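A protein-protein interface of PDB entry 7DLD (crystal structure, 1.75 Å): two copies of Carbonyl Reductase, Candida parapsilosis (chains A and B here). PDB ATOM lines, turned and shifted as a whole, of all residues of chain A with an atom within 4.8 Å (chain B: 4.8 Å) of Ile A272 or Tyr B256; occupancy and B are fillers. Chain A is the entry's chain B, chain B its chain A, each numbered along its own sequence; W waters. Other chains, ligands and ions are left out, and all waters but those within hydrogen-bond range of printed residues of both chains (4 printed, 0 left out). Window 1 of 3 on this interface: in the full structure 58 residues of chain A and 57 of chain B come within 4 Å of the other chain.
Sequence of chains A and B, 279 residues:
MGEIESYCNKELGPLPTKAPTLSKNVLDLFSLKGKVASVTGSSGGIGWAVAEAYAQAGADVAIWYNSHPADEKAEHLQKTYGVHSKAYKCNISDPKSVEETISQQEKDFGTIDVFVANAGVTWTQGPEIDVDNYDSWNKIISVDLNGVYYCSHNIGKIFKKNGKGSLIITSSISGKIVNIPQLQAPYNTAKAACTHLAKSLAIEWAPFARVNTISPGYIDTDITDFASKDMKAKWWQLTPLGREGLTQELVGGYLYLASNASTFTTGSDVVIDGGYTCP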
ATOM      1  N   ILE A 214       2.582  16.476  15.521  1.00  0.00           N
ATOM      2  CA  ILE A 214       1.353  17.243  15.320  1.00  0.00           C
ATOM      3  C   ILE A 214       0.238  16.446  15.979  1.00  0.00           C
ATOM      4  O   ILE A 214       0.138  15.230  15.773  1.00  0.00           O
ATOM      5  CB  ILE A 214       1.044  17.469  13.826  1.00  0.00           C
ATOM      6  CG1 ILE A 214       2.112  18.332  13.147  1.00  0.00           C
ATOM      7  CG2 ILE A 214      -0.378  18.064  13.646  1.00  0.00           C
ATOM      8  CD1 ILE A 214       1.905  19.829  13.248  1.00  0.00           C
ATOM      9  N   SER A 215      -0.583  17.116  16.791  1.00  0.00           N
ATOM     10  CA  SER A 215      -1.729  16.484  17.443  1.00  0.00           C
ATOM     11  C   SER A 215      -2.998  17.168  16.959  1.00  0.00           C
ATOM     12  O   SER A 215      -3.413  18.196  17.519  1.00  0.00           O
ATOM     13  CB  SER A 215      -1.613  16.560  18.963  1.00  0.00           C
ATOM     14  OG  SER A 215      -0.534  15.758  19.399  1.00  0.00           O
ATOM     15  N   PRO A 216      -3.643  16.637  15.930  1.00  0.00           N
ATOM     16  CA  PRO A 216      -4.891  17.239  15.457  1.00  0.00           C
ATOM     17  C   PRO A 216      -6.039  16.963  16.410  1.00  0.00           C
ATOM     18  O   PRO A 216      -6.069  15.949  17.113  1.00  0.00           O
ATOM     19  CB  PRO A 216      -5.133  16.565  14.099  1.00  0.00           C
ATOM     20  CG  PRO A 216      -3.864  15.804  13.787  1.00  0.00           C
ATOM     21  CD  PRO A 216      -3.216  15.499  15.091  1.00  0.00           C
ATOM     22  N   GLY A 217      -6.986  17.894  16.429  1.00  0.00           N
ATOM     23  CA  GLY A 217      -8.242  17.693  17.121  1.00  0.00           C
ATOM     24  C   GLY A 217      -9.217  17.016  16.182  1.00  0.00           C
ATOM     25  O   GLY A 217      -8.824  16.121  15.420  1.00  0.00           O
ATOM     26  N   ILE A 219     -11.028  16.855  12.972  1.00  0.00           N
ATOM     27  CA  ILE A 219     -10.866  17.376  11.624  1.00  0.00           C
ATOM     28  C   ILE A 219     -11.892  16.686  10.740  1.00  0.00           C
ATOM     29  O   ILE A 219     -12.026  15.457  10.777  1.00  0.00           O
ATOM     30  CB  ILE A 219      -9.440  17.142  11.089  1.00  0.00           C
ATOM     31  CG1 ILE A 219      -8.381  17.537  12.128  1.00  0.00           C
ATOM     32  CG2 ILE A 219      -9.227  17.885   9.776  1.00  0.00           C
ATOM     33  CD1 ILE A 219      -8.332  19.020  12.442  1.00  0.00           C
ATOM     34  N   GLU A 249      -6.313  23.666   7.626  1.00  0.00           N
ATOM     35  CA  GLU A 249      -5.870  24.279   8.871  1.00  0.00           C
ATOM     36  C   GLU A 249      -4.771  23.484   9.575  1.00  0.00           C
ATOM     37  O   GLU A 249      -4.272  23.941  10.608  1.00  0.00           O
ATOM     38  CB  GLU A 249      -7.061  24.475   9.808  1.00  0.00           C
ATOM     39  CG  GLU A 249      -8.125  25.412   9.215  1.00  0.00           C
ATOM     40  CD  GLU A 249      -9.358  25.514  10.078  1.00  0.00           C
ATOM     41  OE1 GLU A 249     -10.053  24.488  10.226  1.00  0.00           O
ATOM     42  OE2 GLU A 249      -9.621  26.611  10.613  1.00  0.00           O
ATOM     43  N   LEU A 250      -4.392  22.313   9.053  1.00  0.00           N
ATOM     44  CA  LEU A 250      -3.272  21.546   9.593  1.00  0.00           C
ATOM     45  C   LEU A 250      -1.975  21.748   8.833  1.00  0.00           C
ATOM     46  O   LEU A 250      -0.894  21.605   9.423  1.00  0.00           O
ATOM     47  CB  LEU A 250      -3.589  20.047   9.588  1.00  0.00           C
ATOM     48  CG  LEU A 250      -4.788  19.571  10.408  1.00  0.00           C
ATOM     49  CD1 LEU A 250      -5.108  18.124  10.093  1.00  0.00           C
ATOM     50  CD2 LEU A 250      -4.516  19.744  11.894  1.00  0.00           C
ATOM     51  N   GLY A 252      -0.271  24.205   7.687  1.00  0.00           N
ATOM     52  CA  GLY A 252       0.667  25.208   8.168  1.00  0.00           C
ATOM     53  C   GLY A 252       1.601  24.667   9.235  1.00  0.00           C
ATOM     54  O   GLY A 252       2.813  24.909   9.202  1.00  0.00           O
ATOM     55  N   GLY A 253       1.055  23.919  10.192  1.00  0.00           N
ATOM     56  CA  GLY A 253       1.899  23.330  11.221  1.00  0.00           C
ATOM     57  C   GLY A 253       2.834  22.267  10.675  1.00  0.00           C
ATOM     58  O   GLY A 253       4.004  22.203  11.064  1.00  0.00           O
ATOM     59  N   TYR A 256       5.595  24.031   8.985  1.00  0.00           N
ATOM     60  CA  TYR A 256       6.453  24.642   9.994  1.00  0.00           C
ATOM     61  C   TYR A 256       7.477  23.634  10.518  1.00  0.00           C
ATOM     62  O   TYR A 256       8.689  23.899  10.523  1.00  0.00           O
ATOM     63  CB  TYR A 256       5.590  25.207  11.135  1.00  0.00           C
ATOM     64  CG  TYR A 256       6.406  25.580  12.345  1.00  0.00           C
ATOM     65  CD1 TYR A 256       7.238  26.697  12.327  1.00  0.00           C
ATOM     66  CD2 TYR A 256       6.390  24.786  13.489  1.00  0.00           C
ATOM     67  CE1 TYR A 256       8.017  27.031  13.416  1.00  0.00           C
ATOM     68  CE2 TYR A 256       7.182  25.106  14.597  1.00  0.00           C
ATOM     69  CZ  TYR A 256       7.984  26.234  14.556  1.00  0.00           C
ATOM     70  OH  TYR A 256       8.771  26.564  15.643  1.00  0.00           O
ATOM     71  N   VAL A 270       2.828  19.981  18.675  1.00  0.00           N
ATOM     72  CA  VAL A 270       2.068  21.099  18.126  1.00  0.00           C
ATOM     73  C   VAL A 270       0.601  20.680  18.046  1.00  0.00           C
ATOM     74  O   VAL A 270       0.212  19.881  17.188  1.00  0.00           O
ATOM     75  CB  VAL A 270       2.609  21.527  16.751  1.00  0.00           C
ATOM     76  CG1 VAL A 270       1.756  22.644  16.165  1.00  0.00           C
ATOM     77  CG2 VAL A 270       4.075  21.991  16.870  1.00  0.00           C
ATOM     78  N   VAL A 271      -0.219  21.240  18.932  1.00  0.00           N
ATOM     79  CA  VAL A 271      -1.629  20.887  19.039  1.00  0.00           C
ATOM     80  C   VAL A 271      -2.450  21.792  18.137  1.00  0.00           C
ATOM     81  O   VAL A 271      -2.363  23.023  18.224  1.00  0.00           O
ATOM     82  CB  VAL A 271      -2.107  20.992  20.496  1.00  0.00           C
ATOM     83  CG1 VAL A 271      -3.602  20.707  20.578  1.00  0.00           C
ATOM     84  CG2 VAL A 271      -1.314  20.007  21.367  1.00  0.00           C
ATOM     85  N   ILE A 272      -3.281  21.187  17.296  1.00  0.00           N
ATOM     86  CA  ILE A 272      -4.146  21.928  16.380  1.00  0.00           C
ATOM     87  C   ILE A 272      -5.563  21.392  16.581  1.00  0.00           C
ATOM     88  O   ILE A 272      -6.002  20.461  15.899  1.00  0.00           O
ATOM     89  CB  ILE A 272      -3.692  21.802  14.924  1.00  0.00           C
ATOM     90  CG1 ILE A 272      -2.202  22.122  14.815  1.00  0.00           C
ATOM     91  CG2 ILE A 272      -4.533  22.733  14.014  1.00  0.00           C
ATOM     92  CD1 ILE A 272      -1.605  21.875  13.405  1.00  0.00           C
ATOM     93  N   ASP A 273      -6.298  22.005  17.511  1.00  0.00           N
ATOM     94  CA  ASP A 273      -7.517  21.374  17.993  1.00  0.00           C
ATOM     95  C   ASP A 273      -8.641  22.355  18.310  1.00  0.00           C
ATOM     96  O   ASP A 273      -9.601  21.955  18.963  1.00  0.00           O
ATOM     97  CB  ASP A 273      -7.186  20.528  19.231  1.00  0.00           C
ATOM     98  CG  ASP A 273      -6.858  21.370  20.476  1.00  0.00           C
ATOM     99  OD1 ASP A 273      -6.778  20.763  21.572  1.00  0.00           O
ATOM    100  OD2 ASP A 273      -6.671  22.606  20.377  1.00  0.00           O
ATOM    101  N   GLY A 274      -8.572  23.606  17.870  1.00  0.00           N
ATOM    102  CA  GLY A 274      -9.626  24.541  18.192  1.00  0.00           C
ATOM    103  C   GLY A 274      -9.749  24.821  19.666  1.00  0.00           C
ATOM    104  O   GLY A 274     -10.797  25.290  20.115  1.00  0.00           O
ATOM    105  N   PHE B  30       0.682  32.033   5.133  1.00  0.00           N
ATOM    106  CA  PHE B  30       1.615  32.723   6.007  1.00  0.00           C
ATOM    107  C   PHE B  30       1.762  34.207   5.706  1.00  0.00           C
ATOM    108  O   PHE B  30       2.437  34.911   6.464  1.00  0.00           O
ATOM    109  CB  PHE B  30       2.981  32.052   5.921  1.00  0.00           C
ATOM    110  CG  PHE B  30       3.015  30.689   6.544  1.00  0.00           C
ATOM    111  CD1 PHE B  30       2.657  29.566   5.814  1.00  0.00           C
ATOM    112  CD2 PHE B  30       3.389  30.532   7.869  1.00  0.00           C
ATOM    113  CE1 PHE B  30       2.693  28.313   6.390  1.00  0.00           C
ATOM    114  CE2 PHE B  30       3.413  29.290   8.451  1.00  0.00           C
ATOM    115  CZ  PHE B  30       3.079  28.175   7.712  1.00  0.00           C
ATOM    116  N   GLY B 252       9.668  31.857  12.749  1.00  0.00           N
ATOM    117  CA  GLY B 252       8.736  30.996  12.035  1.00  0.00           C
ATOM    118  C   GLY B 252       7.530  30.617  12.874  1.00  0.00           C
ATOM    119  O   GLY B 252       6.401  30.540  12.370  1.00  0.00           O
ATOM    120  N   GLY B 253       7.748  30.369  14.167  1.00  0.00           N
ATOM    121  CA  GLY B 253       6.630  30.073  15.053  1.00  0.00           C
ATOM    122  C   GLY B 253       5.734  31.276  15.282  1.00  0.00           C
ATOM    123  O   GLY B 253       4.512  31.144  15.364  1.00  0.00           O
ATOM    124  N   TYR B 254       6.329  32.466  15.404  1.00  0.00           N
ATOM    125  CA  TYR B 254       5.538  33.683  15.578  1.00  0.00           C
ATOM    126  C   TYR B 254       4.733  34.007  14.325  1.00  0.00           C
ATOM    127  O   TYR B 254       3.596  34.495  14.415  1.00  0.00           O
ATOM    128  CB  TYR B 254       6.455  34.854  15.941  1.00  0.00           C
ATOM    129  CG  TYR B 254       6.862  34.919  17.399  1.00  0.00           C
ATOM    130  CD1 TYR B 254       8.038  34.321  17.846  1.00  0.00           C
ATOM    131  CD2 TYR B 254       6.074  35.596  18.326  1.00  0.00           C
ATOM    132  CE1 TYR B 254       8.417  34.391  19.170  1.00  0.00           C
ATOM    133  CE2 TYR B 254       6.442  35.677  19.645  1.00  0.00           C
ATOM    134  CZ  TYR B 254       7.624  35.071  20.064  1.00  0.00           C
ATOM    135  OH  TYR B 254       7.983  35.144  21.386  1.00  0.00           O
ATOM    136  N   LEU B 255       5.305  33.746  13.146  1.00  0.00           N
ATOM    137  CA  LEU B 255       4.559  33.924  11.901  1.00  0.00           C
ATOM    138  C   LEU B 255       3.453  32.881  11.770  1.00  0.00           C
ATOM    139  O   LEU B 255       2.335  33.196  11.337  1.00  0.00           O
ATOM    140  CB  LEU B 255       5.520  33.853  10.706  1.00  0.00           C
ATOM    141  CG  LEU B 255       5.338  34.739   9.455  1.00  0.00           C
ATOM    142  CD1 LEU B 255       5.535  33.959   8.144  1.00  0.00           C
ATOM    143  CD2 LEU B 255       4.024  35.491   9.455  1.00  0.00           C
ATOM    144  N   TYR B 256       3.756  31.632  12.136  1.00  0.00           N
ATOM    145  CA  TYR B 256       2.764  30.562  12.127  1.00  0.00           C
ATOM    146  C   TYR B 256       1.507  30.961  12.901  1.00  0.00           C
ATOM    147  O   TYR B 256       0.386  30.843  12.392  1.00  0.00           O
ATOM    148  CB  TYR B 256       3.381  29.283  12.711  1.00  0.00           C
ATOM    149  CG  TYR B 256       2.332  28.233  12.964  1.00  0.00           C
ATOM    150  CD1 TYR B 256       1.698  27.606  11.901  1.00  0.00           C
ATOM    151  CD2 TYR B 256       1.921  27.911  14.266  1.00  0.00           C
ATOM    152  CE1 TYR B 256       0.710  26.672  12.103  1.00  0.00           C
ATOM    153  CE2 TYR B 256       0.917  26.970  14.477  1.00  0.00           C
ATOM    154  CZ  TYR B 256       0.324  26.348  13.386  1.00  0.00           C
ATOM    155  OH  TYR B 256      -0.666  25.409  13.560  1.00  0.00           O
ATOM    156  N   LEU B 257       1.682  31.483  14.119  1.00  0.00           N
ATOM    157  CA  LEU B 257       0.539  31.814  14.970  1.00  0.00           C
ATOM    158  C   LEU B 257      -0.141  33.121  14.565  1.00  0.00           C
ATOM    159  O   LEU B 257      -1.347  33.283  14.799  1.00  0.00           O
ATOM    160  CB  LEU B 257       0.979  31.896  16.436  1.00  0.00           C
ATOM    161  CG  LEU B 257       1.418  30.590  17.100  1.00  0.00           C
ATOM    162  CD1 LEU B 257       1.877  30.847  18.544  1.00  0.00           C
ATOM    163  CD2 LEU B 257       0.273  29.560  17.054  1.00  0.00           C
ATOM    164  N   ALA B 258       0.602  34.048  13.949  1.00  0.00           N
ATOM    165  CA  ALA B 258       0.024  35.343  13.584  1.00  0.00           C
ATOM    166  C   ALA B 258      -0.884  35.247  12.368  1.00  0.00           C
ATOM    167  O   ALA B 258      -1.823  36.046  12.234  1.00  0.00           O
ATOM    168  CB  ALA B 258       1.135  36.364  13.314  1.00  0.00           C
ATOM    169  N   SER B 259      -0.648  34.278  11.496  1.00  0.00           N
ATOM    170  CA  SER B 259      -1.235  34.263  10.164  1.00  0.00           C
ATOM    171  C   SER B 259      -2.353  33.229  10.060  1.00  0.00           C
ATOM    172  O   SER B 259      -2.660  32.492  11.006  1.00  0.00           O
ATOM    173  CB  SER B 259      -0.152  33.976   9.128  1.00  0.00           C
ATOM    174  OG  SER B 259       0.296  32.648   9.273  1.00  0.00           O
ATOM    175  N   ALA B 261      -2.119  30.549   8.748  1.00  0.00           N
ATOM    176  CA  ALA B 261      -1.620  29.189   8.757  1.00  0.00           C
ATOM    177  C   ALA B 261      -2.131  28.408   9.952  1.00  0.00           C
ATOM    178  O   ALA B 261      -2.007  27.185   9.958  1.00  0.00           O
ATOM    179  CB  ALA B 261      -0.089  29.173   8.766  1.00  0.00           C
ATOM    180  N   SER B 262      -2.724  29.084  10.935  1.00  0.00           N
ATOM    181  CA  SER B 262      -3.070  28.479  12.216  1.00  0.00           C
ATOM    182  C   SER B 262      -4.490  28.831  12.649  1.00  0.00           C
ATOM    183  O   SER B 262      -4.756  29.018  13.842  1.00  0.00           O
ATOM    184  CB  SER B 262      -2.069  28.913  13.289  1.00  0.00           C
ATOM    185  OG  SER B 262      -2.082  30.331  13.435  1.00  0.00           O
ATOM    186  N   PHE B 264      -7.119  27.153  13.094  1.00  0.00           N
ATOM    187  CA  PHE B 264      -7.726  26.225  14.039  1.00  0.00           C
ATOM    188  C   PHE B 264      -6.874  26.051  15.292  1.00  0.00           C
ATOM    189  O   PHE B 264      -7.157  25.168  16.114  1.00  0.00           O
ATOM    190  CB  PHE B 264      -7.960  24.870  13.371  1.00  0.00           C
ATOM    191  CG  PHE B 264      -8.979  24.003  14.069  1.00  0.00           C
ATOM    192  CD1 PHE B 264      -8.681  22.680  14.386  1.00  0.00           C
ATOM    193  CD2 PHE B 264     -10.256  24.493  14.362  1.00  0.00           C
ATOM    194  CE1 PHE B 264      -9.626  21.884  15.009  1.00  0.00           C
ATOM    195  CE2 PHE B 264     -11.182  23.699  14.992  1.00  0.00           C
ATOM    196  CZ  PHE B 264     -10.874  22.393  15.315  1.00  0.00           C
ATOM    197  N   THR B 265      -5.858  26.882  15.463  1.00  0.00           N
ATOM    198  CA  THR B 265      -4.905  26.762  16.558  1.00  0.00           C
ATOM    199  C   THR B 265      -5.223  27.830  17.587  1.00  0.00           C
ATOM    200  O   THR B 265      -5.033  29.017  17.334  1.00  0.00           O
ATOM    201  CB  THR B 265      -3.475  26.909  16.056  1.00  0.00           C
ATOM    202  OG1 THR B 265      -3.241  25.968  15.006  1.00  0.00           O
ATOM    203  CG2 THR B 265      -2.467  26.662  17.212  1.00  0.00           C
ATOM    204  N   VAL B 270       3.256  26.829  21.796  1.00  0.00           N
ATOM    205  CA  VAL B 270       4.292  26.398  20.858  1.00  0.00           C
ATOM    206  C   VAL B 270       5.657  26.566  21.531  1.00  0.00           C
ATOM    207  O   VAL B 270       6.152  27.686  21.710  1.00  0.00           O
ATOM    208  CB  VAL B 270       4.221  27.176  19.538  1.00  0.00           C
ATOM    209  CG1 VAL B 270       5.364  26.788  18.627  1.00  0.00           C
ATOM    210  CG2 VAL B 270       2.849  26.944  18.826  1.00  0.00           C
HETATM  211  O   HOH W   1      -4.776  25.827  12.523  1.00  0.00           O
HETATM  212  O   HOH W   2      10.308  28.776  14.871  1.00  0.00           O
HETATM  213  O   HOH W   3      -2.720  25.322   8.062  1.00  0.00           O
HETATM  214  O   HOH W   4      -1.721  24.680  11.087  1.00  0.00           O
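Of the 15 printed residues of chain A, 8 touch a printed residue of chain B.
Printed residues of chain A that touch a printed residue of chain B: Glu A249, Gly A252, Gly A253, Tyr A256, Val A271, Ile A272, Asp A273 and Gly A274.
Of the 14 printed residues of chain B, 7 touch a printed residue of chain A.
Printed residues of chain B that touch a printed residue of chain A: Phe B30, Gly B252, Gly B253, Tyr B256, Ala B261, Phe B264 and Thr B265.
Among the printed residues, 13 pairs touch across the chains.
Among the printed residues, merely in contact across the chains: Glu A249 with Phe B264 (3.6 Å), Gly A252 with Phe B30 (3.6 Å), Gly A252 with Tyr B256 (3.6 Å), Gly A252 with Ala B261 (3.8 Å), Gly A253 with Tyr B256 (3.4 Å), Tyr A256 with Gly B252 (3.7 Å), Tyr A256 with Gly B253 (3.4 Å), Val A271 with Thr B265 (3.8 Å), Ile A272 with Tyr B256 (3.7 Å), Ile A272 with Phe B264 (3.8 Å), Ile A272 with Thr B265 (3.6 Å) and Asp A273 with Phe B264 (3.5 Å).
Gly A252 touches Tyr B256, and with the chains exchanged Tyr A256 touches Gly B252.
Gly A253 touches Tyr B256, and with the chains exchanged Tyr A256 touches Gly B253.
Positions printed for both chains: 252, 253, 256 and 270.
Val A270 touches none of the printed residues of chain B.
Of the printed residues of chain B, Val A271 touches Thr B265 (3.8 Å).
Ile A272 touches just these residues of chain B: Tyr B256, Phe B264 and Thr B265.
Of the printed residues of chain B, Gly A274 touches Phe B264.
Of the printed residues of chain A, Ala B261 touches Gly A252 (3.8 Å).
The nearest printed residue of chain B that does not touch Ile A272 is Ser B262 (6.2 Å).
The nearest residue of chain A that does not touch Tyr B256 is Val A270 (4.5 Å).
Water W4 lies within hydrogen-bond range of the backbone carbonyl oxygen (O) of Glu A249 (2.7 Å), the backbone carbonyl oxygen (O) of Ala B261 (2.8 Å), the side-chain hydroxyl (OH) of Tyr B256 (2.8 Å) and the backbone NH (N) of Gly A253 (3.0 Å).
Water W3 lies within hydrogen-bond range of the backbone NH (N) of Gly A252 (2.7 Å), the backbone carbonyl oxygen (O) of Ala B261 (2.8 Å) and the backbone carbonyl oxygen (O) of Glu A249 (3.3 Å).
Water W1 lies within hydrogen-bond range of the backbone carbonyl oxygen of Glu A249 (2.7 Å), the backbone NH of Phe B264 (2.8 Å), the side-chain hydroxyl of Thr B265 (2.9 Å) and the backbone carbonyl oxygen of Ser B262 (3.5 Å).
Water W2 lies within hydrogen-bond range of OH of Tyr A256 and N of Gly B253.
OG of Ser B262 sits at hydrogen-bond distance from O of Tyr B256 (2.7 Å).
The side-chain hydroxyl of Thr B265 sits at hydrogen-bond distance from the side-chain hydroxyl of Tyr B256 (3.0 Å).
The backbone NH of Ala B261 sits close to the side-chain hydroxyl of Ser B259.
The backbone carbonyl oxygen (O) of Ser A215 lies within hydrogen-bond range of the backbone NH (N) of Ile A272 (3.0 Å).
N of Gly A217 lies within hydrogen-bond range of O of Ile A272, at 2.8 Å.
The backbone carbonyl oxygen (O) of Phe B264 lies within hydrogen-bond range of the backbone NH (N) of Gly A274, 2.7 Å away.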
